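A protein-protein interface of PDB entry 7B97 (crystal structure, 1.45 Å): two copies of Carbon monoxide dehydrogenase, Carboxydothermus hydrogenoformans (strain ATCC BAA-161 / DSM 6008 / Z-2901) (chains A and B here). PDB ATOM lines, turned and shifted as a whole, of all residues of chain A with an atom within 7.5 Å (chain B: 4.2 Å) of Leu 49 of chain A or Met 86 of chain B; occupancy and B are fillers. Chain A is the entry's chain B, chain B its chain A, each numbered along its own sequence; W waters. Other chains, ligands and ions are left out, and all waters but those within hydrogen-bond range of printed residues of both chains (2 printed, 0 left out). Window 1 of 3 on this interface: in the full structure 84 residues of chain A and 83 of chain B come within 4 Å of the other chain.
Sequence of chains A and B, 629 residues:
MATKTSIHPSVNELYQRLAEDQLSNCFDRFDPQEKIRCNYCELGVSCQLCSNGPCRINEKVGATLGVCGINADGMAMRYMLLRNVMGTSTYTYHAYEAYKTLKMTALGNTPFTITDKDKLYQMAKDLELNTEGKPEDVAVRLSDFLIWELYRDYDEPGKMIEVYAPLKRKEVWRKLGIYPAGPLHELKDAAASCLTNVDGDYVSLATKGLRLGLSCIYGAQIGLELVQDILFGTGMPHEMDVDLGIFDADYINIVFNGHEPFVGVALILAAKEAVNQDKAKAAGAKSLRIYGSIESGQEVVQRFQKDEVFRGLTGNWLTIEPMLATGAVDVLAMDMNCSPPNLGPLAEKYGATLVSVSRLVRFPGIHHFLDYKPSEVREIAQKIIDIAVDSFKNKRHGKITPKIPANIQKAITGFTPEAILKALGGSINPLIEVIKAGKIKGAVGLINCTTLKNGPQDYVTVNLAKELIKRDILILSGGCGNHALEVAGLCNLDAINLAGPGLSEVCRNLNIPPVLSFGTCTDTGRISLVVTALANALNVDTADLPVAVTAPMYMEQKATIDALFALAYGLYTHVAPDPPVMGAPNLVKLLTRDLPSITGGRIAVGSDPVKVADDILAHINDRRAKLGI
Leu 49 of chain A touches just these residues of chain B: Tyr 79, Met 86 and Gln 557.
Printed residues of chain B within 4 Å of Leu 82 of chain A: Met 86 (3.8 Å).
Printed residues of chain A within 4 Å of Arg 83 of chain B: Gln 48 (3.1 Å).
Printed residues of chain A within 4 Å of Met 86 of chain B: Leu 49 (3.9 Å), Leu 82 (3.8 Å), Ala 191 (3.4 Å), Cys 194 (3.4 Å) and Leu 195 (3.6 Å).
Gly 87 of chain B touches just one residue of chain A: Leu 195 (3.9 Å).
The nearest printed residue of chain B that does not touch Ala 192 of chain A is Met 86 of chain B (4.4 Å).
Tyr 79 of chain B touches its own counterpart, Tyr 79 of chain A.
3 positions are printed for both chains.
Of the 16 pairs that touch across the chains among the printed residues, 1 has its exchanged pair printed and touching as well.
Along chain A the printed residues that touch a printed residue of chain B span positions 48 to 195.
Of the 11 printed residues of chain B, 7 touch a printed residue of chain A.
The side-chain hydroxyl of Tyr 79 of chain B is in hydrogen-bond range of the side-chain amide oxygen of Gln 48 of chain A (2.6 Å).
SD of Met 86 of chain B lies within hydrogen-bond range of N of Leu 195 of chain A.
The side-chain amide nitrogen (NE2) of Gln 557 of chain B lies within hydrogen-bond range of the backbone carbonyl oxygen (O) of Leu 49 of chain A.
The backbone carbonyl oxygen (O) of Cys 194 of chain A lies close to the side-chain sulfur (SD) of Met 86 of chain B (3.5 Å).
OH of Tyr 79 of chain B lies within hydrogen-bond range of OH of Tyr 79 of chain A (3.1 Å).
The backbone carbonyl oxygen (O) of Gln 48 of chain A sits at hydrogen-bond distance from the guanidinium group (NH2) of Arg 83 of chain B (3.1 Å).
Water W1 lies within hydrogen-bond range of the side-chain amide oxygen (OE1) of Gln 557 of chain B (2.8 Å), the side-chain hydroxyl (OG1) of Thr 196 of chain A (2.8 Å) and the backbone carbonyl oxygen (O) of Leu 49 of chain A (3.0 Å).
Water W2 bridges the side-chain hydroxyl (OH) of Tyr 79 of chain B and the backbone NH (N) of Gln 48 of chain A.
The side-chain sulfur (SG) of Cys 47 of chain A sits close to the backbone NH (N) of Leu 49 of chain A (3.6 Å).
The side-chain sulfur of Cys 194 of chain A is in hydrogen-bond range of the backbone carbonyl oxygen of Ala 190 of chain A.
The side-chain hydroxyl (OG1) of Thr 90 of chain B is in hydrogen-bond range of the backbone carbonyl oxygen (O) of Gly 87 of chain B (2.8 Å).
OG of Ser 46 of chain A lies within hydrogen-bond range of NE2 of Gln 48 of chain A (3.1 Å).
The backbone carbonyl oxygen (O) of Val 85 of chain B sits at hydrogen-bond distance from the side-chain hydroxyl (OG) of Ser 89 of chain B.
O of Arg 78 of chain A lies within hydrogen-bond range of SG of Cys 194 of chain A, 3.4 Å away.
Leu 49 of chain A touches Tyr 79 of chain B.
Met 86 of chain B touches Leu 49 of chain A (CE to CD2, 3.9 Å).
Leu 82 of chain A touches Met 86 of chain B (CD1 to CG, 3.8 Å).
CB of Ser 89 of chain B touches O of Lys 188 of chain A, 3.4 Å away.
Ala 191 of chain A touches Met 86 of chain B.
Ser 89 of chain B touches Ala 191 of chain A.
CB of Ser 89 of chain B touches N of Ala 192 of chain A, at 3.8 Å.
CB of Ala 192 of chain A touches CG2 of Thr 90 of chain B, at 3.8 Å.
CD1 of Leu 195 of chain A touches N of Gly 87 of chain B, 3.9 Å away.
CD1 of Leu 195 of chain A touches OE1 of Gln 557 of chain B, at 3.5 Å.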
ATOM      1  N   SER A  46      22.034 -12.372  -4.979  1.00  0.00           N
ATOM      2  CA  SER A  46      21.548 -12.863  -3.698  1.00  0.00           C
ATOM      3  C   SER A  46      21.751 -14.373  -3.656  1.00  0.00           C
ATOM      4  O   SER A  46      21.886 -15.027  -4.689  1.00  0.00           O
ATOM      5  CB  SER A  46      20.062 -12.568  -3.489  1.00  0.00           C
ATOM      6  OG  SER A  46      19.322 -13.330  -4.407  1.00  0.00           O
ATOM      7  N   CYS A  47      21.775 -14.915  -2.441  1.00  0.00           N
ATOM      8  CA  CYS A  47      21.962 -16.340  -2.244  1.00  0.00           C
ATOM      9  C   CYS A  47      21.192 -16.810  -1.023  1.00  0.00           C
ATOM     10  O   CYS A  47      21.223 -16.176   0.027  1.00  0.00           O
ATOM     11  CB  CYS A  47      23.447 -16.676  -2.103  1.00  0.00           C
ATOM     12  SG  CYS A  47      23.812 -18.430  -2.015  1.00  0.00           S
ATOM     13  N   GLN A  48      20.535 -17.973  -1.163  1.00  0.00           N
ATOM     14  CA  GLN A  48      19.763 -18.551  -0.074  1.00  0.00           C
ATOM     15  C   GLN A  48      20.147 -19.996   0.169  1.00  0.00           C
ATOM     16  O   GLN A  48      19.331 -20.791   0.647  1.00  0.00           O
ATOM     17  CB  GLN A  48      18.271 -18.455  -0.358  1.00  0.00           C
ATOM     18  CG  GLN A  48      17.794 -17.069  -0.694  1.00  0.00           C
ATOM     19  CD  GLN A  48      18.077 -16.665  -2.137  1.00  0.00           C
ATOM     20  OE1 GLN A  48      18.134 -17.501  -3.039  1.00  0.00           O
ATOM     21  NE2 GLN A  48      18.227 -15.354  -2.368  1.00  0.00           N
ATOM     22  N   LEU A  49      21.385 -20.365  -0.132  1.00  0.00           N
ATOM     23  CA  LEU A  49      21.718 -21.790  -0.168  1.00  0.00           C
ATOM     24  C   LEU A  49      22.151 -22.385   1.174  1.00  0.00           C
ATOM     25  O   LEU A  49      22.243 -23.615   1.267  1.00  0.00           O
ATOM     26  CB  LEU A  49      22.805 -22.088  -1.213  1.00  0.00           C
ATOM     27  CG  LEU A  49      22.377 -21.809  -2.662  1.00  0.00           C
ATOM     28  CD1 LEU A  49      23.439 -22.329  -3.588  1.00  0.00           C
ATOM     29  CD2 LEU A  49      20.997 -22.394  -3.019  1.00  0.00           C
ATOM     30  N   CYS A  50      22.418 -21.579   2.203  1.00  0.00           N
ATOM     31  CA  CYS A  50      22.751 -22.128   3.506  1.00  0.00           C
ATOM     32  C   CYS A  50      22.264 -21.203   4.616  1.00  0.00           C
ATOM     33  O   CYS A  50      21.817 -20.079   4.385  1.00  0.00           O
ATOM     34  CB  CYS A  50      24.253 -22.442   3.584  1.00  0.00           C
ATOM     35  SG  CYS A  50      25.275 -21.036   4.124  1.00  0.00           S
ATOM     36  N   SER A  51      22.387 -21.685   5.851  1.00  0.00           N
ATOM     37  CA  SER A  51      21.804 -20.959   6.969  1.00  0.00           C
ATOM     38  C   SER A  51      22.602 -19.734   7.371  1.00  0.00           C
ATOM     39  O   SER A  51      22.076 -18.911   8.125  1.00  0.00           O
ATOM     40  CB  SER A  51      21.692 -21.852   8.198  1.00  0.00           C
ATOM     41  OG  SER A  51      22.974 -22.083   8.756  1.00  0.00           O
ATOM     42  N   ASN A  52      23.863 -19.599   6.939  1.00  0.00           N
ATOM     43  CA  ASN A  52      24.547 -18.328   7.180  1.00  0.00           C
ATOM     44  C   ASN A  52      23.961 -17.190   6.330  1.00  0.00           C
ATOM     45  O   ASN A  52      24.260 -16.023   6.587  1.00  0.00           O
ATOM     46  CB  ASN A  52      26.050 -18.466   6.888  1.00  0.00           C
ATOM     47  CG  ASN A  52      26.862 -18.949   8.103  1.00  0.00           C
ATOM     48  OD1 ASN A  52      26.616 -18.548   9.229  1.00  0.00           O
ATOM     49  ND2 ASN A  52      27.875 -19.755   7.851  1.00  0.00           N
ATOM     50  N   GLY A  53      23.168 -17.519   5.318  1.00  0.00           N
ATOM     51  CA  GLY A  53      22.450 -16.540   4.550  1.00  0.00           C
ATOM     52  C   GLY A  53      21.176 -16.112   5.242  1.00  0.00           C
ATOM     53  O   GLY A  53      20.992 -16.332   6.438  1.00  0.00           O
ATOM     54  N   PRO A  54      20.287 -15.448   4.509  1.00  0.00           N
ATOM     55  CA  PRO A  54      20.427 -15.154   3.081  1.00  0.00           C
ATOM     56  C   PRO A  54      21.486 -14.081   2.878  1.00  0.00           C
ATOM     57  O   PRO A  54      21.562 -13.146   3.701  1.00  0.00           O
ATOM     58  CB  PRO A  54      19.048 -14.640   2.693  1.00  0.00           C
ATOM     59  CG  PRO A  54      18.463 -14.089   3.952  1.00  0.00           C
ATOM     60  CD  PRO A  54      19.015 -14.952   5.068  1.00  0.00           C
ATOM     61  N   CYS A  55      22.258 -14.196   1.801  1.00  0.00           N
ATOM     62  CA  CYS A  55      23.342 -13.261   1.545  1.00  0.00           C
ATOM     63  C   CYS A  55      23.029 -12.410   0.326  1.00  0.00           C
ATOM     64  O   CYS A  55      22.243 -12.797  -0.552  1.00  0.00           O
ATOM     65  CB  CYS A  55      24.675 -13.981   1.295  1.00  0.00           C
ATOM     66  SG  CYS A  55      25.329 -14.793   2.775  1.00  0.00           S
ATOM     67  N   ILE A  70      32.148 -16.768  -1.117  1.00  0.00           N
ATOM     68  CA  ILE A  70      31.908 -16.767  -2.556  1.00  0.00           C
ATOM     69  C   ILE A  70      31.720 -15.347  -3.071  1.00  0.00           C
ATOM     70  O   ILE A  70      31.128 -14.482  -2.392  1.00  0.00           O
ATOM     71  CB  ILE A  70      30.723 -17.673  -2.927  1.00  0.00           C
ATOM     72  CG1 ILE A  70      30.777 -18.039  -4.399  1.00  0.00           C
ATOM     73  CG2 ILE A  70      29.360 -17.033  -2.582  1.00  0.00           C
ATOM     74  CD1 ILE A  70      29.805 -19.176  -4.773  1.00  0.00           C
ATOM     75  N   MET A  75      28.421 -16.797  -7.191  1.00  0.00           N
ATOM     76  CA  MET A  75      27.065 -16.824  -6.673  1.00  0.00           C
ATOM     77  C   MET A  75      26.060 -16.917  -7.808  1.00  0.00           C
ATOM     78  O   MET A  75      25.176 -17.779  -7.800  1.00  0.00           O
ATOM     79  CB  MET A  75      26.827 -15.585  -5.814  1.00  0.00           C
ATOM     80  CG  MET A  75      25.431 -15.491  -5.223  1.00  0.00           C
ATOM     81  SD  MET A  75      25.229 -13.989  -4.217  1.00  0.00           S
ATOM     82  CE  MET A  75      26.340 -14.245  -2.821  1.00  0.00           C
ATOM     83  N   ARG A  78      26.384 -20.197  -9.945  1.00  0.00           N
ATOM     84  CA  ARG A  78      25.978 -21.368  -9.174  1.00  0.00           C
ATOM     85  C   ARG A  78      24.449 -21.511  -9.121  1.00  0.00           C
ATOM     86  O   ARG A  78      23.912 -22.607  -9.296  1.00  0.00           O
ATOM     87  CB  ARG A  78      26.573 -21.295  -7.773  1.00  0.00           C
ATOM     88  CG  ARG A  78      26.190 -22.498  -6.918  1.00  0.00           C
ATOM     89  CD  ARG A  78      26.920 -22.470  -5.604  1.00  0.00           C
ATOM     90  NE  ARG A  78      26.589 -21.283  -4.820  1.00  0.00           N
ATOM     91  CZ  ARG A  78      27.078 -21.013  -3.605  1.00  0.00           C
ATOM     92  NH1 ARG A  78      27.930 -21.854  -3.036  1.00  0.00           N
ATOM     93  NH2 ARG A  78      26.724 -19.897  -2.973  1.00  0.00           N
ATOM     94  N   TYR A  79      23.719 -20.425  -8.853  1.00  0.00           N
ATOM     95  CA  TYR A  79      22.267 -20.551  -8.814  1.00  0.00           C
ATOM     96  C   TYR A  79      21.713 -20.833 -10.207  1.00  0.00           C
ATOM     97  O   TYR A  79      20.773 -21.615 -10.351  1.00  0.00           O
ATOM     98  CB  TYR A  79      21.677 -19.295  -8.193  1.00  0.00           C
ATOM     99  CG  TYR A  79      20.274 -19.349  -7.660  1.00  0.00           C
ATOM    100  CD1 TYR A  79      19.501 -20.511  -7.706  1.00  0.00           C
ATOM    101  CD2 TYR A  79      19.708 -18.219  -7.103  1.00  0.00           C
ATOM    102  CE1 TYR A  79      18.213 -20.526  -7.178  1.00  0.00           C
ATOM    103  CE2 TYR A  79      18.419 -18.207  -6.611  1.00  0.00           C
ATOM    104  CZ  TYR A  79      17.669 -19.371  -6.648  1.00  0.00           C
ATOM    105  OH  TYR A  79      16.383 -19.378  -6.133  1.00  0.00           O
ATOM    106  N   LEU A  82      22.236 -24.572 -10.601  1.00  0.00           N
ATOM    107  CA  LEU A  82      21.264 -25.313  -9.801  1.00  0.00           C
ATOM    108  C   LEU A  82      19.897 -25.315 -10.465  1.00  0.00           C
ATOM    109  O   LEU A  82      19.237 -26.354 -10.551  1.00  0.00           O
ATOM    110  CB  LEU A  82      21.170 -24.712  -8.399  1.00  0.00           C
ATOM    111  CG  LEU A  82      20.065 -25.307  -7.520  1.00  0.00           C
ATOM    112  CD1 LEU A  82      20.330 -26.782  -7.272  1.00  0.00           C
ATOM    113  CD2 LEU A  82      20.016 -24.564  -6.211  1.00  0.00           C
ATOM    114  N   VAL A  85      19.745 -27.716 -13.229  1.00  0.00           N
ATOM    115  CA  VAL A  85      19.529 -29.105 -12.833  1.00  0.00           C
ATOM    116  C   VAL A  85      18.057 -29.459 -12.971  1.00  0.00           C
ATOM    117  O   VAL A  85      17.706 -30.584 -13.361  1.00  0.00           O
ATOM    118  CB  VAL A  85      20.067 -29.330 -11.408  1.00  0.00           C
ATOM    119  CG1 VAL A  85      19.595 -30.668 -10.830  1.00  0.00           C
ATOM    120  CG2 VAL A  85      21.588 -29.213 -11.395  1.00  0.00           C
ATOM    121  N   LYS A 188      23.383 -34.887 -11.287  1.00  0.00           N
ATOM    122  CA  LYS A 188      23.764 -35.133  -9.911  1.00  0.00           C
ATOM    123  C   LYS A 188      25.075 -34.446  -9.571  1.00  0.00           C
ATOM    124  O   LYS A 188      25.215 -33.895  -8.475  1.00  0.00           O
ATOM    125  CB  LYS A 188      23.812 -36.650  -9.669  1.00  0.00           C
ATOM    126  CG  LYS A 188      24.390 -37.106  -8.341  1.00  0.00           C
ATOM    127  CD  LYS A 188      25.867 -37.447  -8.472  1.00  0.00           C
ATOM    128  CE  LYS A 188      26.101 -38.792  -9.131  1.00  0.00           C
ATOM    129  NZ  LYS A 188      27.496 -38.908  -9.720  1.00  0.00           N
ATOM    130  N   ALA A 190      26.330 -31.802 -11.063  1.00  0.00           N
ATOM    131  CA  ALA A 190      26.089 -30.362 -11.035  1.00  0.00           C
ATOM    132  C   ALA A 190      25.419 -29.938  -9.740  1.00  0.00           C
ATOM    133  O   ALA A 190      25.817 -28.947  -9.110  1.00  0.00           O
ATOM    134  CB  ALA A 190      25.249 -29.954 -12.244  1.00  0.00           C
ATOM    135  N   ALA A 191      24.397 -30.682  -9.315  1.00  0.00           N
ATOM    136  CA  ALA A 191      23.723 -30.358  -8.065  1.00  0.00           C
ATOM    137  C   ALA A 191      24.682 -30.443  -6.888  1.00  0.00           C
ATOM    138  O   ALA A 191      24.681 -29.578  -6.016  1.00  0.00           O
ATOM    139  CB  ALA A 191      22.542 -31.306  -7.869  1.00  0.00           C
ATOM    140  N   ALA A 192      25.526 -31.473  -6.854  1.00  0.00           N
ATOM    141  CA  ALA A 192      26.496 -31.608  -5.768  1.00  0.00           C
ATOM    142  C   ALA A 192      27.493 -30.450  -5.767  1.00  0.00           C
ATOM    143  O   ALA A 192      27.898 -29.975  -4.704  1.00  0.00           O
ATOM    144  CB  ALA A 192      27.218 -32.956  -5.870  1.00  0.00           C
ATOM    145  N   SER A 193      27.869 -29.970  -6.954  1.00  0.00           N
ATOM    146  CA  SER A 193      28.804 -28.857  -7.081  1.00  0.00           C
ATOM    147  C   SER A 193      28.219 -27.577  -6.508  1.00  0.00           C
ATOM    148  O   SER A 193      28.962 -26.678  -6.077  1.00  0.00           O
ATOM    149  CB  SER A 193      29.115 -28.620  -8.562  1.00  0.00           C
ATOM    150  OG  SER A 193      29.858 -29.695  -9.131  1.00  0.00           O
ATOM    151  N   CYS A 194      26.900 -27.479  -6.481  1.00  0.00           N
ATOM    152  CA  CYS A 194      26.240 -26.257  -6.049  1.00  0.00           C
ATOM    153  C   CYS A 194      26.032 -26.184  -4.541  1.00  0.00           C
ATOM    154  O   CYS A 194      25.726 -25.115  -4.022  1.00  0.00           O
ATOM    155  CB  CYS A 194      24.896 -26.129  -6.739  1.00  0.00           C
ATOM    156  SG  CYS A 194      24.945 -25.761  -8.504  1.00  0.00           S
ATOM    157  N   LEU A 195      26.209 -27.283  -3.817  1.00  0.00           N
ATOM    158  CA  LEU A 195      26.144 -27.210  -2.372  1.00  0.00           C
ATOM    159  C   LEU A 195      27.197 -26.239  -1.861  1.00  0.00           C
ATOM    160  O   LEU A 195      28.282 -26.108  -2.435  1.00  0.00           O
ATOM    161  CB  LEU A 195      26.348 -28.594  -1.770  1.00  0.00           C
ATOM    162  CG  LEU A 195      25.938 -28.757  -0.315  1.00  0.00           C
ATOM    163  CD1 LEU A 195      24.554 -29.365  -0.214  1.00  0.00           C
ATOM    164  CD2 LEU A 195      26.952 -29.617   0.396  1.00  0.00           C
ATOM    165  N   THR A 196      26.860 -25.569  -0.763  1.00  0.00           N
ATOM    166  CA  THR A 196      27.765 -24.601  -0.156  1.00  0.00           C
ATOM    167  C   THR A 196      29.142 -25.225   0.065  1.00  0.00           C
ATOM    168  O   THR A 196      29.271 -26.385   0.493  1.00  0.00           O
ATOM    169  CB  THR A 196      27.173 -24.142   1.182  1.00  0.00           C
ATOM    170  OG1 THR A 196      25.849 -23.619   0.979  1.00  0.00           O
ATOM    171  CG2 THR A 196      28.040 -23.135   1.853  1.00  0.00           C
ATOM    172  N   TYR B  79      11.414 -24.606  -2.616  1.00  0.00           N
ATOM    173  CA  TYR B  79      12.833 -24.241  -2.578  1.00  0.00           C
ATOM    174  C   TYR B  79      13.573 -25.126  -1.578  1.00  0.00           C
ATOM    175  O   TYR B  79      14.725 -25.499  -1.807  1.00  0.00           O
ATOM    176  CB  TYR B  79      12.989 -22.744  -2.242  1.00  0.00           C
ATOM    177  CG  TYR B  79      14.314 -22.060  -2.599  1.00  0.00           C
ATOM    178  CD1 TYR B  79      15.338 -22.733  -3.244  1.00  0.00           C
ATOM    179  CD2 TYR B  79      14.526 -20.730  -2.247  1.00  0.00           C
ATOM    180  CE1 TYR B  79      16.545 -22.102  -3.530  1.00  0.00           C
ATOM    181  CE2 TYR B  79      15.706 -20.076  -2.554  1.00  0.00           C
ATOM    182  CZ  TYR B  79      16.718 -20.754  -3.197  1.00  0.00           C
ATOM    183  OH  TYR B  79      17.903 -20.102  -3.472  1.00  0.00           O
ATOM    184  N   LEU B  82      14.248 -28.310  -3.556  1.00  0.00           N
ATOM    185  CA  LEU B  82      15.333 -28.090  -4.518  1.00  0.00           C
ATOM    186  C   LEU B  82      16.692 -28.091  -3.840  1.00  0.00           C
ATOM    187  O   LEU B  82      17.644 -28.727  -4.320  1.00  0.00           O
ATOM    188  CB  LEU B  82      15.109 -26.772  -5.263  1.00  0.00           C
ATOM    189  CG  LEU B  82      16.211 -26.405  -6.248  1.00  0.00           C
ATOM    190  CD1 LEU B  82      16.356 -27.452  -7.351  1.00  0.00           C
ATOM    191  CD2 LEU B  82      15.924 -25.019  -6.857  1.00  0.00           C
ATOM    192  N   ARG B  83      16.822 -27.369  -2.732  1.00  0.00           N
ATOM    193  CA  ARG B  83      18.115 -27.371  -2.058  1.00  0.00           C
ATOM    194  C   ARG B  83      18.464 -28.769  -1.569  1.00  0.00           C
ATOM    195  O   ARG B  83      19.634 -29.179  -1.615  1.00  0.00           O
ATOM    196  CB  ARG B  83      18.138 -26.342  -0.930  1.00  0.00           C
ATOM    197  CG  ARG B  83      18.135 -24.883  -1.421  1.00  0.00           C
ATOM    198  CD  ARG B  83      18.261 -23.894  -0.226  1.00  0.00           C
ATOM    199  NE  ARG B  83      17.000 -23.946   0.492  1.00  0.00           N
ATOM    200  CZ  ARG B  83      16.138 -22.948   0.655  1.00  0.00           C
ATOM    201  NH1 ARG B  83      14.994 -23.190   1.259  1.00  0.00           N
ATOM    202  NH2 ARG B  83      16.440 -21.713   0.325  1.00  0.00           N
ATOM    203  N   ASN B  84      17.457 -29.539  -1.165  1.00  0.00           N
ATOM    204  CA  ASN B  84      17.735 -30.885  -0.682  1.00  0.00           C
ATOM    205  C   ASN B  84      18.092 -31.853  -1.802  1.00  0.00           C
ATOM    206  O   ASN B  84      18.680 -32.892  -1.520  1.00  0.00           O
ATOM    207  CB  ASN B  84      16.611 -31.382   0.227  1.00  0.00           C
ATOM    208  CG  ASN B  84      16.777 -30.879   1.632  1.00  0.00           C
ATOM    209  OD1 ASN B  84      17.415 -31.509   2.456  1.00  0.00           O
ATOM    210  ND2 ASN B  84      16.266 -29.685   1.891  1.00  0.00           N
ATOM    211  N   VAL B  85      17.783 -31.530  -3.054  1.00  0.00           N
ATOM    212  CA  VAL B  85      18.389 -32.250  -4.161  1.00  0.00           C
ATOM    213  C   VAL B  85      19.908 -32.166  -4.079  1.00  0.00           C
ATOM    214  O   VAL B  85      20.611 -33.134  -4.380  1.00  0.00           O
ATOM    215  CB  VAL B  85      17.848 -31.722  -5.510  1.00  0.00           C
ATOM    216  CG1 VAL B  85      18.657 -32.299  -6.673  1.00  0.00           C
ATOM    217  CG2 VAL B  85      16.356 -32.077  -5.650  1.00  0.00           C
ATOM    218  N   MET B  86      20.449 -31.000  -3.712  1.00  0.00           N
ATOM    219  CA  MET B  86      21.900 -30.895  -3.601  1.00  0.00           C
ATOM    220  C   MET B  86      22.424 -31.825  -2.512  1.00  0.00           C
ATOM    221  O   MET B  86      23.439 -32.506  -2.687  1.00  0.00           O
ATOM    222  CB  MET B  86      22.323 -29.463  -3.265  1.00  0.00           C
ATOM    223  CG  MET B  86      21.948 -28.413  -4.300  1.00  0.00           C
ATOM    224  SD  MET B  86      22.689 -26.804  -3.966  1.00  0.00           S
ATOM    225  CE  MET B  86      21.718 -26.232  -2.588  1.00  0.00           C
ATOM    226  N   GLY B  87      21.769 -31.820  -1.357  1.00  0.00           N
ATOM    227  CA  GLY B  87      22.199 -32.681  -0.273  1.00  0.00           C
ATOM    228  C   GLY B  87      22.192 -34.143  -0.682  1.00  0.00           C
ATOM    229  O   GLY B  87      23.173 -34.870  -0.472  1.00  0.00           O
ATOM    230  N   THR B  88      21.090 -34.582  -1.297  1.00  0.00           N
ATOM    231  CA  THR B  88      20.981 -35.973  -1.730  1.00  0.00           C
ATOM    232  C   THR B  88      22.043 -36.290  -2.772  1.00  0.00           C
ATOM    233  O   THR B  88      22.631 -37.371  -2.759  1.00  0.00           O
ATOM    234  CB  THR B  88      19.578 -36.238  -2.300  1.00  0.00           C
ATOM    235  OG1 THR B  88      18.580 -35.912  -1.319  1.00  0.00           O
ATOM    236  CG2 THR B  88      19.419 -37.691  -2.675  1.00  0.00           C
ATOM    237  N   SER B  89      22.287 -35.352  -3.692  1.00  0.00           N
ATOM    238  CA  SER B  89      23.273 -35.574  -4.741  1.00  0.00           C
ATOM    239  C   SER B  89      24.658 -35.802  -4.160  1.00  0.00           C
ATOM    240  O   SER B  89      25.415 -36.608  -4.694  1.00  0.00           O
ATOM    241  CB  SER B  89      23.301 -34.407  -5.730  1.00  0.00           C
ATOM    242  OG  SER B  89      22.110 -34.330  -6.496  1.00  0.00           O
ATOM    243  N   THR B  90      25.034 -35.058  -3.109  1.00  0.00           N
ATOM    244  CA  THR B  90      26.355 -35.240  -2.518  1.00  0.00           C
ATOM    245  C   THR B  90      26.481 -36.625  -1.889  1.00  0.00           C
ATOM    246  O   THR B  90      27.490 -37.300  -2.079  1.00  0.00           O
ATOM    247  CB  THR B  90      26.707 -34.143  -1.496  1.00  0.00           C
ATOM    248  OG1 THR B  90      25.885 -34.235  -0.328  1.00  0.00           O
ATOM    249  CG2 THR B  90      26.601 -32.775  -2.093  1.00  0.00           C
ATOM    250  N   GLN B 557      22.315 -28.717   3.299  1.00  0.00           N
ATOM    251  CA  GLN B 557      21.333 -29.766   3.101  1.00  0.00           C
ATOM    252  C   GLN B 557      21.877 -31.175   3.288  1.00  0.00           C
ATOM    253  O   GLN B 557      21.106 -32.128   3.192  1.00  0.00           O
ATOM    254  CB  GLN B 557      20.660 -29.578   1.749  1.00  0.00           C
ATOM    255  CG  GLN B 557      19.943 -28.228   1.645  1.00  0.00           C
ATOM    256  CD  GLN B 557      20.902 -27.060   1.425  1.00  0.00           C
ATOM    257  OE1 GLN B 557      21.942 -27.247   0.827  1.00  0.00           O
ATOM    258  NE2 GLN B 557      20.548 -25.874   1.915  1.00  0.00           N
HETATM  259  O   HOH W   1      24.116 -25.653   0.181  1.00  0.00           O
HETATM  260  O   HOH W   2      20.612 -19.016  -3.951  1.00  0.00           O
